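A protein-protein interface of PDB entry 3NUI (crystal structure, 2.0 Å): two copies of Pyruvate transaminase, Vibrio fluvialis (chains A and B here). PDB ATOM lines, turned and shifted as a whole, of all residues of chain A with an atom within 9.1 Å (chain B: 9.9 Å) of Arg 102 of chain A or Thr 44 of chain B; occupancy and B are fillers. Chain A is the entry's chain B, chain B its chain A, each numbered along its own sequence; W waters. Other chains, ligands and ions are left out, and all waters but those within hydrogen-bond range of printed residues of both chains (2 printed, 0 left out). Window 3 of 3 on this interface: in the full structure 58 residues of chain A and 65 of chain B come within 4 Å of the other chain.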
ATOM      1  N   PRO A  94      31.739   4.450 -18.319  1.00  0.00           N
ATOM      2  CA  PRO A  94      30.638   5.412 -18.402  1.00  0.00           C
ATOM      3  C   PRO A  94      30.313   5.772 -19.834  1.00  0.00           C
ATOM      4  O   PRO A  94      31.145   5.588 -20.719  1.00  0.00           O
ATOM      5  CB  PRO A  94      31.213   6.670 -17.695  1.00  0.00           C
ATOM      6  CG  PRO A  94      32.336   6.133 -16.832  1.00  0.00           C
ATOM      7  CD  PRO A  94      32.902   4.978 -17.588  1.00  0.00           C
ATOM      8  N   GLY A  95      29.126   6.336 -20.058  1.00  0.00           N
ATOM      9  CA  GLY A  95      28.798   6.890 -21.381  1.00  0.00           C
ATOM     10  C   GLY A  95      29.391   8.294 -21.455  1.00  0.00           C
ATOM     11  O   GLY A  95      28.678   9.302 -21.617  1.00  0.00           O
ATOM     12  N   TYR A  96      30.702   8.361 -21.331  1.00  0.00           N
ATOM     13  CA  TYR A  96      31.354   9.667 -21.268  1.00  0.00           C
ATOM     14  C   TYR A  96      31.409  10.365 -22.618  1.00  0.00           C
ATOM     15  O   TYR A  96      31.834   9.798 -23.622  1.00  0.00           O
ATOM     16  CB  TYR A  96      32.715   9.512 -20.656  1.00  0.00           C
ATOM     17  CG  TYR A  96      33.538  10.789 -20.543  1.00  0.00           C
ATOM     18  CD1 TYR A  96      32.991  11.966 -20.065  1.00  0.00           C
ATOM     19  CD2 TYR A  96      34.907  10.750 -20.841  1.00  0.00           C
ATOM     20  CE1 TYR A  96      33.808  13.110 -19.877  1.00  0.00           C
ATOM     21  CE2 TYR A  96      35.711  11.890 -20.695  1.00  0.00           C
ATOM     22  CZ  TYR A  96      35.134  13.052 -20.226  1.00  0.00           C
ATOM     23  OH  TYR A  96      35.938  14.148 -20.075  1.00  0.00           O
ATOM     24  N   HIS A  97      30.851  11.575 -22.666  1.00  0.00           N
ATOM     25  CA  HIS A  97      30.663  12.252 -23.953  1.00  0.00           C
ATOM     26  C   HIS A  97      31.148  13.694 -23.912  1.00  0.00           C
ATOM     27  O   HIS A  97      31.147  14.310 -22.851  1.00  0.00           O
ATOM     28  CB  HIS A  97      29.181  12.255 -24.230  1.00  0.00           C
ATOM     29  CG  HIS A  97      28.835  12.379 -25.664  1.00  0.00           C
ATOM     30  ND1 HIS A  97      28.648  13.597 -26.268  1.00  0.00           N
ATOM     31  CD2 HIS A  97      28.643  11.443 -26.618  1.00  0.00           C
ATOM     32  CE1 HIS A  97      28.390  13.413 -27.558  1.00  0.00           C
ATOM     33  NE2 HIS A  97      28.381  12.116 -27.800  1.00  0.00           N
ATOM     34  N   PHE A  99      29.534  16.310 -25.098  1.00  0.00           N
ATOM     35  CA  PHE A  99      28.432  17.249 -24.867  1.00  0.00           C
ATOM     36  C   PHE A  99      27.100  16.579 -24.509  1.00  0.00           C
ATOM     37  O   PHE A  99      26.338  17.169 -23.870  1.00  0.00           O
ATOM     38  CB  PHE A  99      28.312  18.289 -25.991  1.00  0.00           C
ATOM     39  CG  PHE A  99      28.088  17.692 -27.336  1.00  0.00           C
ATOM     40  CD1 PHE A  99      26.825  17.422 -27.786  1.00  0.00           C
ATOM     41  CD2 PHE A  99      29.136  17.315 -28.110  1.00  0.00           C
ATOM     42  CE1 PHE A  99      26.634  16.824 -28.995  1.00  0.00           C
ATOM     43  CE2 PHE A  99      28.946  16.718 -29.311  1.00  0.00           C
ATOM     44  CZ  PHE A  99      27.697  16.492 -29.749  1.00  0.00           C
ATOM     45  N   PHE A 100      26.810  15.403 -24.924  1.00  0.00           N
ATOM     46  CA  PHE A 100      25.543  14.790 -24.619  1.00  0.00           C
ATOM     47  C   PHE A 100      25.345  14.174 -23.229  1.00  0.00           C
ATOM     48  O   PHE A 100      26.122  13.372 -22.813  1.00  0.00           O
ATOM     49  CB  PHE A 100      25.204  13.784 -25.700  1.00  0.00           C
ATOM     50  CG  PHE A 100      23.856  13.207 -25.568  1.00  0.00           C
ATOM     51  CD1 PHE A 100      22.773  13.861 -26.025  1.00  0.00           C
ATOM     52  CD2 PHE A 100      23.659  12.043 -24.912  1.00  0.00           C
ATOM     53  CE1 PHE A 100      21.534  13.336 -25.872  1.00  0.00           C
ATOM     54  CE2 PHE A 100      22.422  11.539 -24.779  1.00  0.00           C
ATOM     55  CZ  PHE A 100      21.372  12.194 -25.271  1.00  0.00           C
ATOM     56  N   GLY A 101      24.266  14.567 -22.569  1.00  0.00           N
ATOM     57  CA  GLY A 101      23.881  13.841 -21.331  1.00  0.00           C
ATOM     58  C   GLY A 101      24.323  14.622 -20.109  1.00  0.00           C
ATOM     59  O   GLY A 101      25.242  15.464 -20.178  1.00  0.00           O
ATOM     60  N   ARG A 102      23.690  14.355 -18.989  1.00  0.00           N
ATOM     61  CA  ARG A 102      24.087  15.018 -17.726  1.00  0.00           C
ATOM     62  C   ARG A 102      25.427  14.563 -17.227  1.00  0.00           C
ATOM     63  O   ARG A 102      25.778  13.424 -17.464  1.00  0.00           O
ATOM     64  CB  ARG A 102      23.065  14.692 -16.655  1.00  0.00           C
ATOM     65  CG  ARG A 102      21.979  15.687 -16.641  1.00  0.00           C
ATOM     66  CD  ARG A 102      21.295  15.646 -15.284  1.00  0.00           C
ATOM     67  NE  ARG A 102      19.888  15.454 -15.546  1.00  0.00           N
ATOM     68  CZ  ARG A 102      19.036  14.846 -14.728  1.00  0.00           C
ATOM     69  NH1 ARG A 102      19.445  14.343 -13.564  1.00  0.00           N
ATOM     70  NH2 ARG A 102      17.765  14.711 -15.110  1.00  0.00           N
ATOM     71  N   MET A 103      26.129  15.419 -16.449  1.00  0.00           N
ATOM     72  CA  MET A 103      27.375  14.999 -15.793  1.00  0.00           C
ATOM     73  C   MET A 103      27.088  13.790 -14.941  1.00  0.00           C
ATOM     74  O   MET A 103      26.015  13.711 -14.371  1.00  0.00           O
ATOM     75  CB  MET A 103      27.964  16.127 -14.912  1.00  0.00           C
ATOM     76  CG  MET A 103      28.495  17.283 -15.718  1.00  0.00           C
ATOM     77  SD  MET A 103      29.470  18.310 -14.574  1.00  0.00           S
ATOM     78  CE  MET A 103      28.106  19.043 -13.600  1.00  0.00           C
ATOM     79  N   SER A 104      28.014  12.831 -14.921  1.00  0.00           N
ATOM     80  CA  SER A 104      27.859  11.608 -14.163  1.00  0.00           C
ATOM     81  C   SER A 104      27.834  11.888 -12.676  1.00  0.00           C
ATOM     82  O   SER A 104      28.393  12.869 -12.166  1.00  0.00           O
ATOM     83  CB  SER A 104      29.025  10.628 -14.418  1.00  0.00           C
ATOM     84  OG  SER A 104      30.225  11.108 -13.791  1.00  0.00           O
ATOM     85  N   ASP A 105      27.151  11.010 -11.984  1.00  0.00           N
ATOM     86  CA  ASP A 105      27.134  11.059 -10.549  1.00  0.00           C
ATOM     87  C   ASP A 105      28.514  11.144  -9.923  1.00  0.00           C
ATOM     88  O   ASP A 105      28.674  11.941  -9.016  1.00  0.00           O
ATOM     89  CB  ASP A 105      26.293   9.905 -10.025  1.00  0.00           C
ATOM     90  CG  ASP A 105      24.848   9.987 -10.539  1.00  0.00           C
ATOM     91  OD1 ASP A 105      24.179  11.014 -10.291  1.00  0.00           O
ATOM     92  OD2 ASP A 105      24.421   9.068 -11.266  1.00  0.00           O
ATOM     93  N   GLN A 106      29.503  10.352 -10.392  1.00  0.00           N
ATOM     94  CA  GLN A 106      30.898  10.385  -9.850  1.00  0.00           C
ATOM     95  C   GLN A 106      31.538  11.781  -9.895  1.00  0.00           C
ATOM     96  O   GLN A 106      32.201  12.229  -8.987  1.00  0.00           O
ATOM     97  CB  GLN A 106      31.847   9.492 -10.681  1.00  0.00           C
ATOM     98  CG  GLN A 106      31.442   8.078 -10.752  1.00  0.00           C
ATOM     99  CD  GLN A 106      30.856   7.732 -12.083  1.00  0.00           C
ATOM    100  OE1 GLN A 106      29.824   8.277 -12.486  1.00  0.00           O
ATOM    101  NE2 GLN A 106      31.521   6.826 -12.792  1.00  0.00           N
ATOM    102  N   THR A 107      31.377  12.428 -11.026  1.00  0.00           N
ATOM    103  CA  THR A 107      31.923  13.748 -11.201  1.00  0.00           C
ATOM    104  C   THR A 107      31.297  14.782 -10.229  1.00  0.00           C
ATOM    105  O   THR A 107      32.029  15.519  -9.541  1.00  0.00           O
ATOM    106  CB  THR A 107      31.648  14.154 -12.631  1.00  0.00           C
ATOM    107  OG1 THR A 107      32.038  13.042 -13.500  1.00  0.00           O
ATOM    108  CG2 THR A 107      32.386  15.435 -12.929  1.00  0.00           C
ATOM    109  N   VAL A 108      29.956  14.828 -10.148  1.00  0.00           N
ATOM    110  CA  VAL A 108      29.293  15.714  -9.191  1.00  0.00           C
ATOM    111  C   VAL A 108      29.804  15.443  -7.775  1.00  0.00           C
ATOM    112  O   VAL A 108      30.161  16.358  -7.012  1.00  0.00           O
ATOM    113  CB  VAL A 108      27.764  15.522  -9.256  1.00  0.00           C
ATOM    114  CG1 VAL A 108      27.069  16.398  -8.253  1.00  0.00           C
ATOM    115  CG2 VAL A 108      27.273  15.815 -10.673  1.00  0.00           C
ATOM    116  N   SER A 338      32.996  19.058 -16.037  1.00  0.00           N
ATOM    117  CA  SER A 338      32.752  17.677 -16.253  1.00  0.00           C
ATOM    118  C   SER A 338      34.092  16.877 -16.319  1.00  0.00           C
ATOM    119  O   SER A 338      34.654  16.681 -17.417  1.00  0.00           O
ATOM    120  CB  SER A 338      31.922  17.551 -17.528  1.00  0.00           C
ATOM    121  OG  SER A 338      31.679  16.173 -17.813  1.00  0.00           O
ATOM    122  N   GLY A 339      34.602  16.419 -15.172  1.00  0.00           N
ATOM    123  CA  GLY A 339      35.863  15.642 -15.151  1.00  0.00           C
ATOM    124  C   GLY A 339      35.651  14.231 -15.653  1.00  0.00           C
ATOM    125  O   GLY A 339      34.512  13.750 -15.690  1.00  0.00           O
ATOM    126  N   PRO A 341      34.803  10.576 -15.894  1.00  0.00           N
ATOM    127  CA  PRO A 341      34.135   9.912 -14.758  1.00  0.00           C
ATOM    128  C   PRO A 341      34.873   8.770 -14.158  1.00  0.00           C
ATOM    129  O   PRO A 341      34.712   8.497 -12.961  1.00  0.00           O
ATOM    130  CB  PRO A 341      32.771   9.443 -15.315  1.00  0.00           C
ATOM    131  CG  PRO A 341      32.838   9.601 -16.775  1.00  0.00           C
ATOM    132  CD  PRO A 341      33.939  10.665 -17.084  1.00  0.00           C
ATOM    133  N   THR B  44      19.918  17.357 -19.442  1.00  0.00           N
ATOM    134  CA  THR B  44      18.609  16.755 -19.035  1.00  0.00           C
ATOM    135  C   THR B  44      18.588  15.204 -19.137  1.00  0.00           C
ATOM    136  O   THR B  44      17.841  14.556 -18.411  1.00  0.00           O
ATOM    137  CB  THR B  44      17.415  17.255 -19.917  1.00  0.00           C
ATOM    138  OG1 THR B  44      17.648  16.883 -21.292  1.00  0.00           O
ATOM    139  CG2 THR B  44      17.162  18.785 -19.824  1.00  0.00           C
ATOM    140  N   VAL B  45      19.325  14.599 -20.068  1.00  0.00           N
ATOM    141  CA  VAL B  45      19.245  13.153 -20.245  1.00  0.00           C
ATOM    142  C   VAL B  45      20.286  12.454 -19.347  1.00  0.00           C
ATOM    143  O   VAL B  45      21.462  12.808 -19.391  1.00  0.00           O
ATOM    144  CB  VAL B  45      19.425  12.782 -21.763  1.00  0.00           C
ATOM    145  CG1 VAL B  45      19.732  11.325 -21.945  1.00  0.00           C
ATOM    146  CG2 VAL B  45      18.171  13.204 -22.557  1.00  0.00           C
ATOM    147  N   VAL B  46      19.851  11.504 -18.520  1.00  0.00           N
ATOM    148  CA  VAL B  46      20.768  10.734 -17.622  1.00  0.00           C
ATOM    149  C   VAL B  46      21.337   9.527 -18.306  1.00  0.00           C
ATOM    150  O   VAL B  46      20.588   8.636 -18.759  1.00  0.00           O
ATOM    151  CB  VAL B  46      20.122  10.252 -16.289  1.00  0.00           C
ATOM    152  CG1 VAL B  46      21.193   9.643 -15.353  1.00  0.00           C
ATOM    153  CG2 VAL B  46      19.379  11.421 -15.567  1.00  0.00           C
ATOM    154  N   VAL B  47      22.661   9.503 -18.407  1.00  0.00           N
ATOM    155  CA  VAL B  47      23.369   8.457 -19.127  1.00  0.00           C
ATOM    156  C   VAL B  47      24.346   7.735 -18.220  1.00  0.00           C
ATOM    157  O   VAL B  47      25.185   8.371 -17.563  1.00  0.00           O
ATOM    158  CB  VAL B  47      24.114   9.042 -20.356  1.00  0.00           C
ATOM    159  CG1 VAL B  47      25.063   7.971 -20.961  1.00  0.00           C
ATOM    160  CG2 VAL B  47      23.066   9.593 -21.433  1.00  0.00           C
ATOM    161  N   THR B  48      24.268   6.409 -18.146  1.00  0.00           N
ATOM    162  CA  THR B  48      25.222   5.691 -17.272  1.00  0.00           C
ATOM    163  C   THR B  48      26.236   4.859 -18.021  1.00  0.00           C
ATOM    164  O   THR B  48      27.182   4.315 -17.422  1.00  0.00           O
ATOM    165  CB  THR B  48      24.497   4.778 -16.216  1.00  0.00           C
ATOM    166  OG1 THR B  48      23.983   3.639 -16.872  1.00  0.00           O
ATOM    167  CG2 THR B  48      23.338   5.531 -15.452  1.00  0.00           C
ATOM    168  N   HIS B  49      26.028   4.653 -19.331  1.00  0.00           N
ATOM    169  CA  HIS B  49      26.953   3.787 -20.048  1.00  0.00           C
ATOM    170  C   HIS B  49      26.580   3.813 -21.534  1.00  0.00           C
ATOM    171  O   HIS B  49      25.598   4.521 -21.925  1.00  0.00           O
ATOM    172  CB  HIS B  49      26.702   2.360 -19.612  1.00  0.00           C
ATOM    173  CG  HIS B  49      25.315   1.871 -19.907  1.00  0.00           C
ATOM    174  ND1 HIS B  49      25.045   0.879 -20.825  1.00  0.00           N
ATOM    175  CD2 HIS B  49      24.125   2.196 -19.350  1.00  0.00           C
ATOM    176  CE1 HIS B  49      23.748   0.613 -20.824  1.00  0.00           C
ATOM    177  NE2 HIS B  49      23.170   1.403 -19.934  1.00  0.00           N
ATOM    178  N   ILE B  55      24.925   5.615 -27.085  1.00  0.00           N
ATOM    179  CA  ILE B  55      24.901   6.135 -25.740  1.00  0.00           C
ATOM    180  C   ILE B  55      23.545   5.638 -25.262  1.00  0.00           C
ATOM    181  O   ILE B  55      22.634   5.665 -26.034  1.00  0.00           O
ATOM    182  CB  ILE B  55      24.886   7.660 -25.810  1.00  0.00           C
ATOM    183  CG1 ILE B  55      26.332   8.214 -25.880  1.00  0.00           C
ATOM    184  CG2 ILE B  55      24.194   8.274 -24.602  1.00  0.00           C
ATOM    185  CD1 ILE B  55      27.208   7.970 -24.612  1.00  0.00           C
ATOM    186  N   VAL B  56      23.432   5.116 -24.032  1.00  0.00           N
ATOM    187  CA  VAL B  56      22.133   4.562 -23.538  1.00  0.00           C
ATOM    188  C   VAL B  56      21.679   5.380 -22.340  1.00  0.00           C
ATOM    189  O   VAL B  56      22.439   5.506 -21.354  1.00  0.00           O
ATOM    190  CB  VAL B  56      22.332   3.145 -23.076  1.00  0.00           C
ATOM    191  CG1 VAL B  56      20.925   2.460 -22.714  1.00  0.00           C
ATOM    192  CG2 VAL B  56      22.950   2.370 -24.241  1.00  0.00           C
ATOM    193  N   ASP B  57      20.452   5.895 -22.371  1.00  0.00           N
ATOM    194  CA  ASP B  57      19.983   6.617 -21.171  1.00  0.00           C
ATOM    195  C   ASP B  57      19.349   5.649 -20.130  1.00  0.00           C
ATOM    196  O   ASP B  57      19.175   4.457 -20.446  1.00  0.00           O
ATOM    197  CB  ASP B  57      19.051   7.808 -21.531  1.00  0.00           C
ATOM    198  CG  ASP B  57      17.627   7.420 -21.952  1.00  0.00           C
ATOM    199  OD1 ASP B  57      17.121   6.295 -21.735  1.00  0.00           O
ATOM    200  OD2 ASP B  57      16.941   8.321 -22.540  1.00  0.00           O
ATOM    201  N   VAL B  58      19.058   6.136 -18.924  1.00  0.00           N
ATOM    202  CA  VAL B  58      18.612   5.248 -17.829  1.00  0.00           C
ATOM    203  C   VAL B  58      17.327   4.514 -18.224  1.00  0.00           C
ATOM    204  O   VAL B  58      17.070   3.450 -17.698  1.00  0.00           O
ATOM    205  CB  VAL B  58      18.422   5.983 -16.454  1.00  0.00           C
ATOM    206  CG1 VAL B  58      19.749   6.380 -15.908  1.00  0.00           C
ATOM    207  CG2 VAL B  58      17.463   7.242 -16.576  1.00  0.00           C
ATOM    208  N   ASN B  59      16.527   5.067 -19.160  1.00  0.00           N
ATOM    209  CA  ASN B  59      15.245   4.425 -19.570  1.00  0.00           C
ATOM    210  C   ASN B  59      15.499   3.395 -20.647  1.00  0.00           C
ATOM    211  O   ASN B  59      14.605   2.662 -21.007  1.00  0.00           O
ATOM    212  CB  ASN B  59      14.191   5.417 -20.105  1.00  0.00           C
ATOM    213  CG  ASN B  59      13.826   6.479 -19.141  1.00  0.00           C
ATOM    214  OD1 ASN B  59      13.927   6.279 -17.935  1.00  0.00           O
ATOM    215  ND2 ASN B  59      13.367   7.670 -19.669  1.00  0.00           N
ATOM    216  N   TYR B  63      21.029   6.209 -28.364  1.00  0.00           N
ATOM    217  CA  TYR B  63      21.291   7.383 -29.228  1.00  0.00           C
ATOM    218  C   TYR B  63      22.554   7.024 -29.965  1.00  0.00           C
ATOM    219  O   TYR B  63      23.623   6.919 -29.351  1.00  0.00           O
ATOM    220  CB  TYR B  63      21.523   8.652 -28.393  1.00  0.00           C
ATOM    221  CG  TYR B  63      20.361   8.995 -27.415  1.00  0.00           C
ATOM    222  CD1 TYR B  63      19.514  10.057 -27.668  1.00  0.00           C
ATOM    223  CD2 TYR B  63      20.176   8.256 -26.224  1.00  0.00           C
ATOM    224  CE1 TYR B  63      18.428  10.418 -26.762  1.00  0.00           C
ATOM    225  CE2 TYR B  63      19.154   8.612 -25.295  1.00  0.00           C
ATOM    226  CZ  TYR B  63      18.303   9.689 -25.569  1.00  0.00           C
ATOM    227  OH  TYR B  63      17.286   9.953 -24.699  1.00  0.00           O
ATOM    228  N   ASN B 419      19.930  19.396 -31.898  1.00  0.00           N
ATOM    229  CA  ASN B 419      18.879  19.117 -30.922  1.00  0.00           C
ATOM    230  C   ASN B 419      17.814  18.214 -31.450  1.00  0.00           C
ATOM    231  O   ASN B 419      17.342  17.322 -30.732  1.00  0.00           O
ATOM    232  CB  ASN B 419      18.248  20.372 -30.311  1.00  0.00           C
ATOM    233  CG  ASN B 419      19.237  21.154 -29.457  1.00  0.00           C
ATOM    234  OD1 ASN B 419      20.273  20.626 -29.038  1.00  0.00           O
ATOM    235  ND2 ASN B 419      18.952  22.411 -29.233  1.00  0.00           N
ATOM    236  N   THR B 422      19.034  14.570 -31.562  1.00  0.00           N
ATOM    237  CA  THR B 422      18.932  13.974 -30.200  1.00  0.00           C
ATOM    238  C   THR B 422      17.479  13.463 -29.923  1.00  0.00           C
ATOM    239  O   THR B 422      17.264  12.301 -29.490  1.00  0.00           O
ATOM    240  CB  THR B 422      19.446  15.077 -29.249  1.00  0.00           C
ATOM    241  OG1 THR B 422      20.909  15.020 -29.226  1.00  0.00           O
ATOM    242  CG2 THR B 422      18.914  14.975 -27.974  1.00  0.00           C
ATOM    243  N   ASP B 423      16.483  14.284 -30.269  1.00  0.00           N
ATOM    244  CA  ASP B 423      15.069  13.908 -30.121  1.00  0.00           C
ATOM    245  C   ASP B 423      14.736  12.656 -30.901  1.00  0.00           C
ATOM    246  O   ASP B 423      13.858  11.870 -30.495  1.00  0.00           O
ATOM    247  CB  ASP B 423      14.145  14.989 -30.670  1.00  0.00           C
ATOM    248  CG  ASP B 423      14.150  16.240 -29.864  1.00  0.00           C
ATOM    249  OD1 ASP B 423      14.581  16.227 -28.683  1.00  0.00           O
ATOM    250  OD2 ASP B 423      13.681  17.270 -30.423  1.00  0.00           O
HETATM  251  O   HOH W   1      27.929   7.712 -17.727  1.00  0.00           O
HETATM  252  O   HOH W   2      24.503  11.189 -16.964  1.00  0.00           O
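The backbone carbonyl oxygen of Thr 44 of chain B lies within hydrogen-bond range of the guanidinium group of Arg 102 of chain A (3.3 Å).
The backbone NH of Arg 102 of chain A is in hydrogen-bond range of the backbone carbonyl oxygen of Val 45 of chain B (2.7 Å).
The backbone NH (N) of Val 58 of chain B is in hydrogen-bond range of the backbone carbonyl oxygen (O) of Val 46 of chain B (2.9 Å).
The backbone carbonyl oxygen (O) of His 49 of chain B lies within hydrogen-bond range of the backbone NH (N) of Val 56 of chain B (3.1 Å).
N of Tyr 63 of chain B lies within hydrogen-bond range of O of Ile 55 of chain B, at 2.9 Å.
OH of Tyr 63 of chain B sits at hydrogen-bond distance from OD2 of Asp 57 of chain B.
N of Phe 100 of chain A sits at hydrogen-bond distance from ND1 of His 97 of chain A.
Among the printed residues, pairs that only touch across the chains: Pro 94 of chain A with Thr 48 of chain B (3.8 Å), Pro 94 of chain A with His 49 of chain B (3.9 Å), Gly 95 of chain A with Val 47 of chain B (3.9 Å), Gly 95 of chain A with Thr 48 of chain B (3.8 Å), Gly 95 of chain A with His 49 of chain B (3.3 Å), Gly 95 of chain A with Ile 55 of chain B (3.6 Å), Phe 100 of chain A with Val 45 of chain B (3.8 Å), Phe 100 of chain A with Val 47 of chain B (3.9 Å), Phe 100 of chain A with Ile 55 of chain B (3.7 Å), Phe 100 of chain A with Tyr 63 of chain B (3.7 Å), Phe 100 of chain A with Thr 422 of chain B (3.7 Å), Gly 101 of chain A with Val 45 of chain B (3.3 Å) and Arg 102 of chain A with Val 46 of chain B (3.5 Å).
Printed residues of chain B within 4 Å of Pro 94 of chain A: Thr 48 and His 49.
Printed residues of chain B within 4 Å of Phe 100 of chain A: Val 45, Val 47, Ile 55, Tyr 63 and Thr 422.
Gly 101 of chain A touches one residue of chain B.
Of chain B, only Thr 44 (3.3 Å), Val 45 (2.7 Å) and Val 46 (3.5 Å) come within 4 Å of Arg 102 of chain A.
Thr 44 of chain B touches just one residue of chain A: Arg 102.
Val 45 of chain B touches three residues of chain A.
The nearest residue of chain B that does not touch Arg 102 of chain A is Val 47 of chain B (5.0 Å).
The nearest residue of chain A that does not touch Thr 44 of chain B is Gly 101 of chain A (5.2 Å).
Printed residues of chain B that touch a printed residue of chain A: Thr 44, Val 45, Val 46, Val 47, Thr 48, His 49, Ile 55, Tyr 63 and Thr 422.
Hydrophobic or aromatic side chains of chain B within 4 Å of the printed part of chain A: Val 45, Val 46, Val 47, Ile 55 and Tyr 63.
Printed residues of chain A that touch a printed residue of chain B: Pro 94, Gly 95, Phe 100, Gly 101 and Arg 102.
Hydrophobic or aromatic side chains of chain A that line the printed part of chain B: Phe 100.
Among the printed residues, no Asp or Glu carboxylate lies within 4 Å of a Lys or Arg side-chain nitrogen of the other chain.
No position is printed for both chains.
Water W2 lies within hydrogen-bond range of O of Arg 102 of chain A (2.6 Å) and N of Val 47 of chain B (2.9 Å).
Water W1 lies within hydrogen-bond range of O of Val 47 of chain B (2.8 Å), N of Gly 95 of chain A (3.0 Å) and O of Thr 48 of chain B (3.5 Å).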
